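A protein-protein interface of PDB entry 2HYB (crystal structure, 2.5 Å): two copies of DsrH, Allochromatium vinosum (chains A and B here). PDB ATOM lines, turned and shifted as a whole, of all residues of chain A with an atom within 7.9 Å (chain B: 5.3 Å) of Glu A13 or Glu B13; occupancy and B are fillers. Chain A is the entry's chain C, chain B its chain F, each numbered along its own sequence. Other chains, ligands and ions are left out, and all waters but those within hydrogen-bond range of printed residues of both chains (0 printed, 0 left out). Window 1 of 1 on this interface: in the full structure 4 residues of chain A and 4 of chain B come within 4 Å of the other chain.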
ATOM      1  N   LYS A   9      10.002 -34.660   0.744  1.00  0.00           N
ATOM      2  CA  LYS A   9       9.800 -33.364   1.386  1.00  0.00           C
ATOM      3  C   LYS A   9       9.684 -32.160   0.441  1.00  0.00           C
ATOM      4  O   LYS A   9      10.313 -32.130  -0.612  1.00  0.00           O
ATOM      5  CB  LYS A   9      10.911 -33.128   2.410  1.00  0.00           C
ATOM      6  CG  LYS A   9      10.421 -33.119   3.848  1.00  0.00           C
ATOM      7  CD  LYS A   9       9.779 -34.436   4.230  1.00  0.00           C
ATOM      8  CE  LYS A   9       9.123 -34.351   5.595  1.00  0.00           C
ATOM      9  NZ  LYS A   9       8.033 -33.330   5.642  1.00  0.00           N
ATOM     10  N   SER A  10       8.884 -31.167   0.840  1.00  0.00           N
ATOM     11  CA  SER A  10       8.657 -29.949   0.046  1.00  0.00           C
ATOM     12  C   SER A  10       9.931 -29.185  -0.243  1.00  0.00           C
ATOM     13  O   SER A  10      10.685 -28.863   0.666  1.00  0.00           O
ATOM     14  CB  SER A  10       7.676 -29.012   0.758  1.00  0.00           C
ATOM     15  OG  SER A  10       7.589 -27.773   0.079  1.00  0.00           O
ATOM     16  N   PRO A  11      10.161 -28.833  -1.514  1.00  0.00           N
ATOM     17  CA  PRO A  11      11.379 -28.102  -1.853  1.00  0.00           C
ATOM     18  C   PRO A  11      11.415 -26.690  -1.271  1.00  0.00           C
ATOM     19  O   PRO A  11      12.448 -26.017  -1.334  1.00  0.00           O
ATOM     20  CB  PRO A  11      11.357 -28.100  -3.370  1.00  0.00           C
ATOM     21  CG  PRO A  11       9.906 -27.904  -3.649  1.00  0.00           C
ATOM     22  CD  PRO A  11       9.225 -28.834  -2.653  1.00  0.00           C
ATOM     23  N   PHE A  12      10.297 -26.243  -0.701  1.00  0.00           N
ATOM     24  CA  PHE A  12      10.228 -24.899  -0.128  1.00  0.00           C
ATOM     25  C   PHE A  12      10.456 -24.921   1.375  1.00  0.00           C
ATOM     26  O   PHE A  12      10.562 -23.879   2.024  1.00  0.00           O
ATOM     27  CB  PHE A  12       8.874 -24.261  -0.454  1.00  0.00           C
ATOM     28  CG  PHE A  12       8.462 -24.446  -1.877  1.00  0.00           C
ATOM     29  CD1 PHE A  12       7.454 -25.348  -2.215  1.00  0.00           C
ATOM     30  CD2 PHE A  12       9.127 -23.774  -2.893  1.00  0.00           C
ATOM     31  CE1 PHE A  12       7.119 -25.582  -3.555  1.00  0.00           C
ATOM     32  CE2 PHE A  12       8.805 -23.997  -4.241  1.00  0.00           C
ATOM     33  CZ  PHE A  12       7.802 -24.902  -4.571  1.00  0.00           C
ATOM     34  N   GLU A  13      10.555 -26.124   1.921  1.00  0.00           N
ATOM     35  CA  GLU A  13      10.761 -26.292   3.350  1.00  0.00           C
ATOM     36  C   GLU A  13      12.092 -26.992   3.636  1.00  0.00           C
ATOM     37  O   GLU A  13      12.815 -26.599   4.550  1.00  0.00           O
ATOM     38  CB  GLU A  13       9.582 -27.076   3.932  1.00  0.00           C
ATOM     39  CG  GLU A  13       9.743 -27.556   5.348  1.00  0.00           C
ATOM     40  CD  GLU A  13       8.473 -28.202   5.869  1.00  0.00           C
ATOM     41  OE1 GLU A  13       8.569 -29.075   6.756  1.00  0.00           O
ATOM     42  OE2 GLU A  13       7.376 -27.825   5.403  1.00  0.00           O
ATOM     43  N   ARG A  14      12.428 -27.993   2.819  1.00  0.00           N
ATOM     44  CA  ARG A  14      13.660 -28.766   2.977  1.00  0.00           C
ATOM     45  C   ARG A  14      14.647 -28.672   1.806  1.00  0.00           C
ATOM     46  O   ARG A  14      14.255 -28.520   0.660  1.00  0.00           O
ATOM     47  CB  ARG A  14      13.317 -30.238   3.186  1.00  0.00           C
ATOM     48  CG  ARG A  14      13.594 -30.775   4.572  1.00  0.00           C
ATOM     49  CD  ARG A  14      12.389 -30.656   5.455  1.00  0.00           C
ATOM     50  NE  ARG A  14      12.484 -31.566   6.587  1.00  0.00           N
ATOM     51  CZ  ARG A  14      11.470 -31.851   7.394  1.00  0.00           C
ATOM     52  NH1 ARG A  14      10.280 -31.295   7.191  1.00  0.00           N
ATOM     53  NH2 ARG A  14      11.640 -32.699   8.399  1.00  0.00           N
ATOM     54  N   ASN A  15      15.930 -28.802   2.122  1.00  0.00           N
ATOM     55  CA  ASN A  15      17.026 -28.764   1.155  1.00  0.00           C
ATOM     56  C   ASN A  15      17.199 -30.139   0.510  1.00  0.00           C
ATOM     57  O   ASN A  15      18.116 -30.345  -0.280  1.00  0.00           O
ATOM     58  CB  ASN A  15      18.324 -28.436   1.881  1.00  0.00           C
ATOM     59  CG  ASN A  15      18.773 -29.577   2.806  1.00  0.00           C
ATOM     60  OD1 ASN A  15      18.010 -30.046   3.654  1.00  0.00           O
ATOM     61  ND2 ASN A  15      20.010 -30.023   2.637  1.00  0.00           N
ATOM     62  N   SER A  16      16.337 -31.083   0.862  1.00  0.00           N
ATOM     63  CA  SER A  16      16.439 -32.430   0.331  1.00  0.00           C
ATOM     64  C   SER A  16      16.407 -32.520  -1.174  1.00  0.00           C
ATOM     65  O   SER A  16      17.206 -33.237  -1.765  1.00  0.00           O
ATOM     66  CB  SER A  16      15.332 -33.317   0.899  1.00  0.00           C
ATOM     67  OG  SER A  16      15.463 -33.451   2.299  1.00  0.00           O
ATOM     68  N   ASP A  35       5.004 -34.889   0.607  1.00  0.00           N
ATOM     69  CA  ASP A  35       5.146 -33.457   0.363  1.00  0.00           C
ATOM     70  C   ASP A  35       6.151 -33.127  -0.755  1.00  0.00           C
ATOM     71  O   ASP A  35       6.249 -31.978  -1.201  1.00  0.00           O
ATOM     72  CB  ASP A  35       5.512 -32.739   1.669  1.00  0.00           C
ATOM     73  CG  ASP A  35       4.370 -32.749   2.676  1.00  0.00           C
ATOM     74  OD1 ASP A  35       4.551 -32.285   3.826  1.00  0.00           O
ATOM     75  OD2 ASP A  35       3.284 -33.227   2.298  1.00  0.00           O
ATOM     76  N   TYR A  38       5.060 -31.139  -4.509  1.00  0.00           N
ATOM     77  CA  TYR A  38       5.055 -29.754  -4.934  1.00  0.00           C
ATOM     78  C   TYR A  38       6.182 -29.347  -5.904  1.00  0.00           C
ATOM     79  O   TYR A  38       6.052 -28.377  -6.656  1.00  0.00           O
ATOM     80  CB  TYR A  38       5.035 -28.860  -3.703  1.00  0.00           C
ATOM     81  CG  TYR A  38       3.845 -29.135  -2.811  1.00  0.00           C
ATOM     82  CD1 TYR A  38       4.024 -29.620  -1.524  1.00  0.00           C
ATOM     83  CD2 TYR A  38       2.535 -28.870  -3.244  1.00  0.00           C
ATOM     84  CE1 TYR A  38       2.933 -29.830  -0.677  1.00  0.00           C
ATOM     85  CE2 TYR A  38       1.442 -29.071  -2.407  1.00  0.00           C
ATOM     86  CZ  TYR A  38       1.649 -29.549  -1.116  1.00  0.00           C
ATOM     87  OH  TYR A  38       0.602 -29.699  -0.233  1.00  0.00           O
ATOM     88  N   ARG A  45       8.819 -21.599  -7.869  1.00  0.00           N
ATOM     89  CA  ARG A  45      10.150 -21.033  -7.774  1.00  0.00           C
ATOM     90  C   ARG A  45      11.226 -21.999  -8.285  1.00  0.00           C
ATOM     91  O   ARG A  45      12.249 -21.569  -8.813  1.00  0.00           O
ATOM     92  CB  ARG A  45      10.413 -20.724  -6.306  1.00  0.00           C
ATOM     93  CG  ARG A  45      11.372 -19.603  -6.039  1.00  0.00           C
ATOM     94  CD  ARG A  45      11.535 -19.447  -4.556  1.00  0.00           C
ATOM     95  NE  ARG A  45      12.035 -20.684  -3.985  1.00  0.00           N
ATOM     96  CZ  ARG A  45      11.773 -21.082  -2.753  1.00  0.00           C
ATOM     97  NH1 ARG A  45      11.010 -20.334  -1.967  1.00  0.00           N
ATOM     98  NH2 ARG A  45      12.274 -22.223  -2.309  1.00  0.00           N
ATOM     99  N   LEU A 102      15.654 -37.880   3.078  1.00  0.00           N
ATOM    100  CA  LEU A 102      14.717 -37.455   4.105  1.00  0.00           C
ATOM    101  C   LEU A 102      15.031 -36.087   4.716  1.00  0.00           C
ATOM    102  O   LEU A 102      16.222 -35.731   4.829  1.00  0.00           O
ATOM    103  CB  LEU A 102      14.681 -38.518   5.208  1.00  0.00           C
ATOM    104  CG  LEU A 102      14.499 -39.985   4.789  1.00  0.00           C
ATOM    105  CD1 LEU A 102      14.855 -40.899   5.963  1.00  0.00           C
ATOM    106  CD2 LEU A 102      13.075 -40.226   4.319  1.00  0.00           C
ATOM    107  N   LYS B   9      15.310 -24.468  14.073  1.00  0.00           N
ATOM    108  CA  LYS B   9      15.816 -25.319  13.005  1.00  0.00           C
ATOM    109  C   LYS B   9      17.011 -24.752  12.246  1.00  0.00           C
ATOM    110  O   LYS B   9      17.176 -23.539  12.123  1.00  0.00           O
ATOM    111  CB  LYS B   9      14.682 -25.654  12.023  1.00  0.00           C
ATOM    112  CG  LYS B   9      14.214 -27.104  12.082  1.00  0.00           C
ATOM    113  CD  LYS B   9      13.855 -27.518  13.496  1.00  0.00           C
ATOM    114  CE  LYS B   9      13.542 -29.010  13.575  1.00  0.00           C
ATOM    115  NZ  LYS B   9      14.714 -29.886  13.266  1.00  0.00           N
ATOM    116  N   SER B  10      17.833 -25.670  11.745  1.00  0.00           N
ATOM    117  CA  SER B  10      19.044 -25.381  10.981  1.00  0.00           C
ATOM    118  C   SER B  10      18.686 -24.572   9.728  1.00  0.00           C
ATOM    119  O   SER B  10      17.714 -24.892   9.041  1.00  0.00           O
ATOM    120  CB  SER B  10      19.690 -26.728  10.596  1.00  0.00           C
ATOM    121  OG  SER B  10      20.933 -26.595   9.936  1.00  0.00           O
ATOM    122  N   PRO B  11      19.461 -23.511   9.416  1.00  0.00           N
ATOM    123  CA  PRO B  11      19.203 -22.677   8.240  1.00  0.00           C
ATOM    124  C   PRO B  11      19.665 -23.363   6.975  1.00  0.00           C
ATOM    125  O   PRO B  11      19.481 -22.845   5.881  1.00  0.00           O
ATOM    126  CB  PRO B  11      20.021 -21.432   8.527  1.00  0.00           C
ATOM    127  CG  PRO B  11      21.216 -22.000   9.199  1.00  0.00           C
ATOM    128  CD  PRO B  11      20.587 -22.954  10.187  1.00  0.00           C
ATOM    129  N   PHE B  12      20.282 -24.527   7.124  1.00  0.00           N
ATOM    130  CA  PHE B  12      20.762 -25.252   5.963  1.00  0.00           C
ATOM    131  C   PHE B  12      19.813 -26.397   5.662  1.00  0.00           C
ATOM    132  O   PHE B  12      19.956 -27.085   4.645  1.00  0.00           O
ATOM    133  CB  PHE B  12      22.178 -25.787   6.205  1.00  0.00           C
ATOM    134  CG  PHE B  12      23.105 -24.779   6.812  1.00  0.00           C
ATOM    135  CD1 PHE B  12      23.399 -24.819   8.170  1.00  0.00           C
ATOM    136  CD2 PHE B  12      23.642 -23.759   6.046  1.00  0.00           C
ATOM    137  CE1 PHE B  12      24.211 -23.852   8.765  1.00  0.00           C
ATOM    138  CE2 PHE B  12      24.455 -22.784   6.633  1.00  0.00           C
ATOM    139  CZ  PHE B  12      24.738 -22.834   7.995  1.00  0.00           C
ATOM    140  N   GLU B  13      18.842 -26.605   6.550  1.00  0.00           N
ATOM    141  CA  GLU B  13      17.849 -27.668   6.374  1.00  0.00           C
ATOM    142  C   GLU B  13      16.416 -27.133   6.204  1.00  0.00           C
ATOM    143  O   GLU B  13      15.631 -27.693   5.444  1.00  0.00           O
ATOM    144  CB  GLU B  13      17.894 -28.640   7.564  1.00  0.00           C
ATOM    145  CG  GLU B  13      16.678 -29.570   7.654  1.00  0.00           C
ATOM    146  CD  GLU B  13      16.794 -30.640   8.736  1.00  0.00           C
ATOM    147  OE1 GLU B  13      15.746 -31.189   9.139  1.00  0.00           O
ATOM    148  OE2 GLU B  13      17.927 -30.943   9.172  1.00  0.00           O
ATOM    149  N   ARG B  14      16.091 -26.049   6.907  1.00  0.00           N
ATOM    150  CA  ARG B  14      14.760 -25.448   6.862  1.00  0.00           C
ATOM    151  C   ARG B  14      14.787 -23.978   6.445  1.00  0.00           C
ATOM    152  O   ARG B  14      15.802 -23.289   6.573  1.00  0.00           O
ATOM    153  CB  ARG B  14      14.095 -25.538   8.236  1.00  0.00           C
ATOM    154  CG  ARG B  14      12.895 -26.453   8.322  1.00  0.00           C
ATOM    155  CD  ARG B  14      13.300 -27.854   8.703  1.00  0.00           C
ATOM    156  NE  ARG B  14      12.182 -28.591   9.283  1.00  0.00           N
ATOM    157  CZ  ARG B  14      12.300 -29.756   9.910  1.00  0.00           C
ATOM    158  NH1 ARG B  14      13.492 -30.322  10.040  1.00  0.00           N
ATOM    159  NH2 ARG B  14      11.228 -30.350  10.417  1.00  0.00           N
ATOM    160  N   ASN B  15      13.634 -23.507   5.983  1.00  0.00           N
ATOM    161  CA  ASN B  15      13.454 -22.137   5.526  1.00  0.00           C
ATOM    162  C   ASN B  15      12.953 -21.243   6.667  1.00  0.00           C
ATOM    163  O   ASN B  15      12.709 -20.046   6.477  1.00  0.00           O
ATOM    164  CB  ASN B  15      12.439 -22.114   4.381  1.00  0.00           C
ATOM    165  CG  ASN B  15      11.032 -22.492   4.840  1.00  0.00           C
ATOM    166  OD1 ASN B  15      10.801 -23.591   5.356  1.00  0.00           O
ATOM    167  ND2 ASN B  15      10.087 -21.575   4.664  1.00  0.00           N
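NH2 of Arg B14 sits close to NH2 of Arg A14 (3.1 Å). O of Phe A12 lies close to OD1 of Asn B15 (3.4 Å). The backbone carbonyl oxygen of Glu A13 lies close to the backbone carbonyl oxygen of Glu B13, at 3.2 Å.
Glu A13 touches just these residues of chain B: Glu B13, Arg B14 and Asn B15. Glu B13 touches three residues of chain A. Printed residues of chain B within 4 Å of Phe A12: Asn B15. Printed residues of chain A within 4 Å of Phe B12: Asn A15. Printed residues of chain A within 4 Å of Asn B15: Phe A12 and Glu A13. Printed residues of chain A within 4 Å of Arg B14: Glu A13 (3.2 Å) and Arg A14 (3.1 Å). Pro A11 touches none of the printed residues of chain B. Tyr A38 touches none of the printed residues of chain B.
Of the 12 printed residues of chain A, 4 touch a printed residue of chain B. Of the 7 printed residues of chain B, 4 touch a printed residue of chain A. Printed residues of chain B that touch a printed residue of chain A: Phe B12, Glu B13, Arg B14 and Asn B15. Among the printed residues, 8 pairs touch across the chains. Among the printed residues, no Asp or Glu carboxylate lies within 4 Å of a Lys or Arg side-chain nitrogen of the other chain.
The guanidinium group (NH1) of Arg A14 is in salt-bridge range of the side-chain carboxylate (OE1) of Glu A13 (2.8 Å). OG of Ser A10 lies close to N of Phe A12 (3.2 Å). The side-chain carboxylate of Glu B13 lies within salt-bridge range of the guanidinium group of Arg B14, 2.6 Å away.
Among the printed residues, pairs that only touch across the chains: Glu A13 with Arg B14, Asn A15 with Phe B12, Arg A14 with Glu B13, Glu A13 with Asn B15 and Asn A15 with Glu B13.
Phe A12 touches Asn B15, and with the chains exchanged Asn A15 touches Phe B12. Glu B13 touches its own counterpart, Glu A13. Glu A13 touches Arg B14, and with the chains exchanged Arg A14 touches Glu B13. Arg A14 touches its own counterpart, Arg B14. Of the 8 pairs that touch across the chains among the printed residues, 8 have their exchanged pair printed and touching as well.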
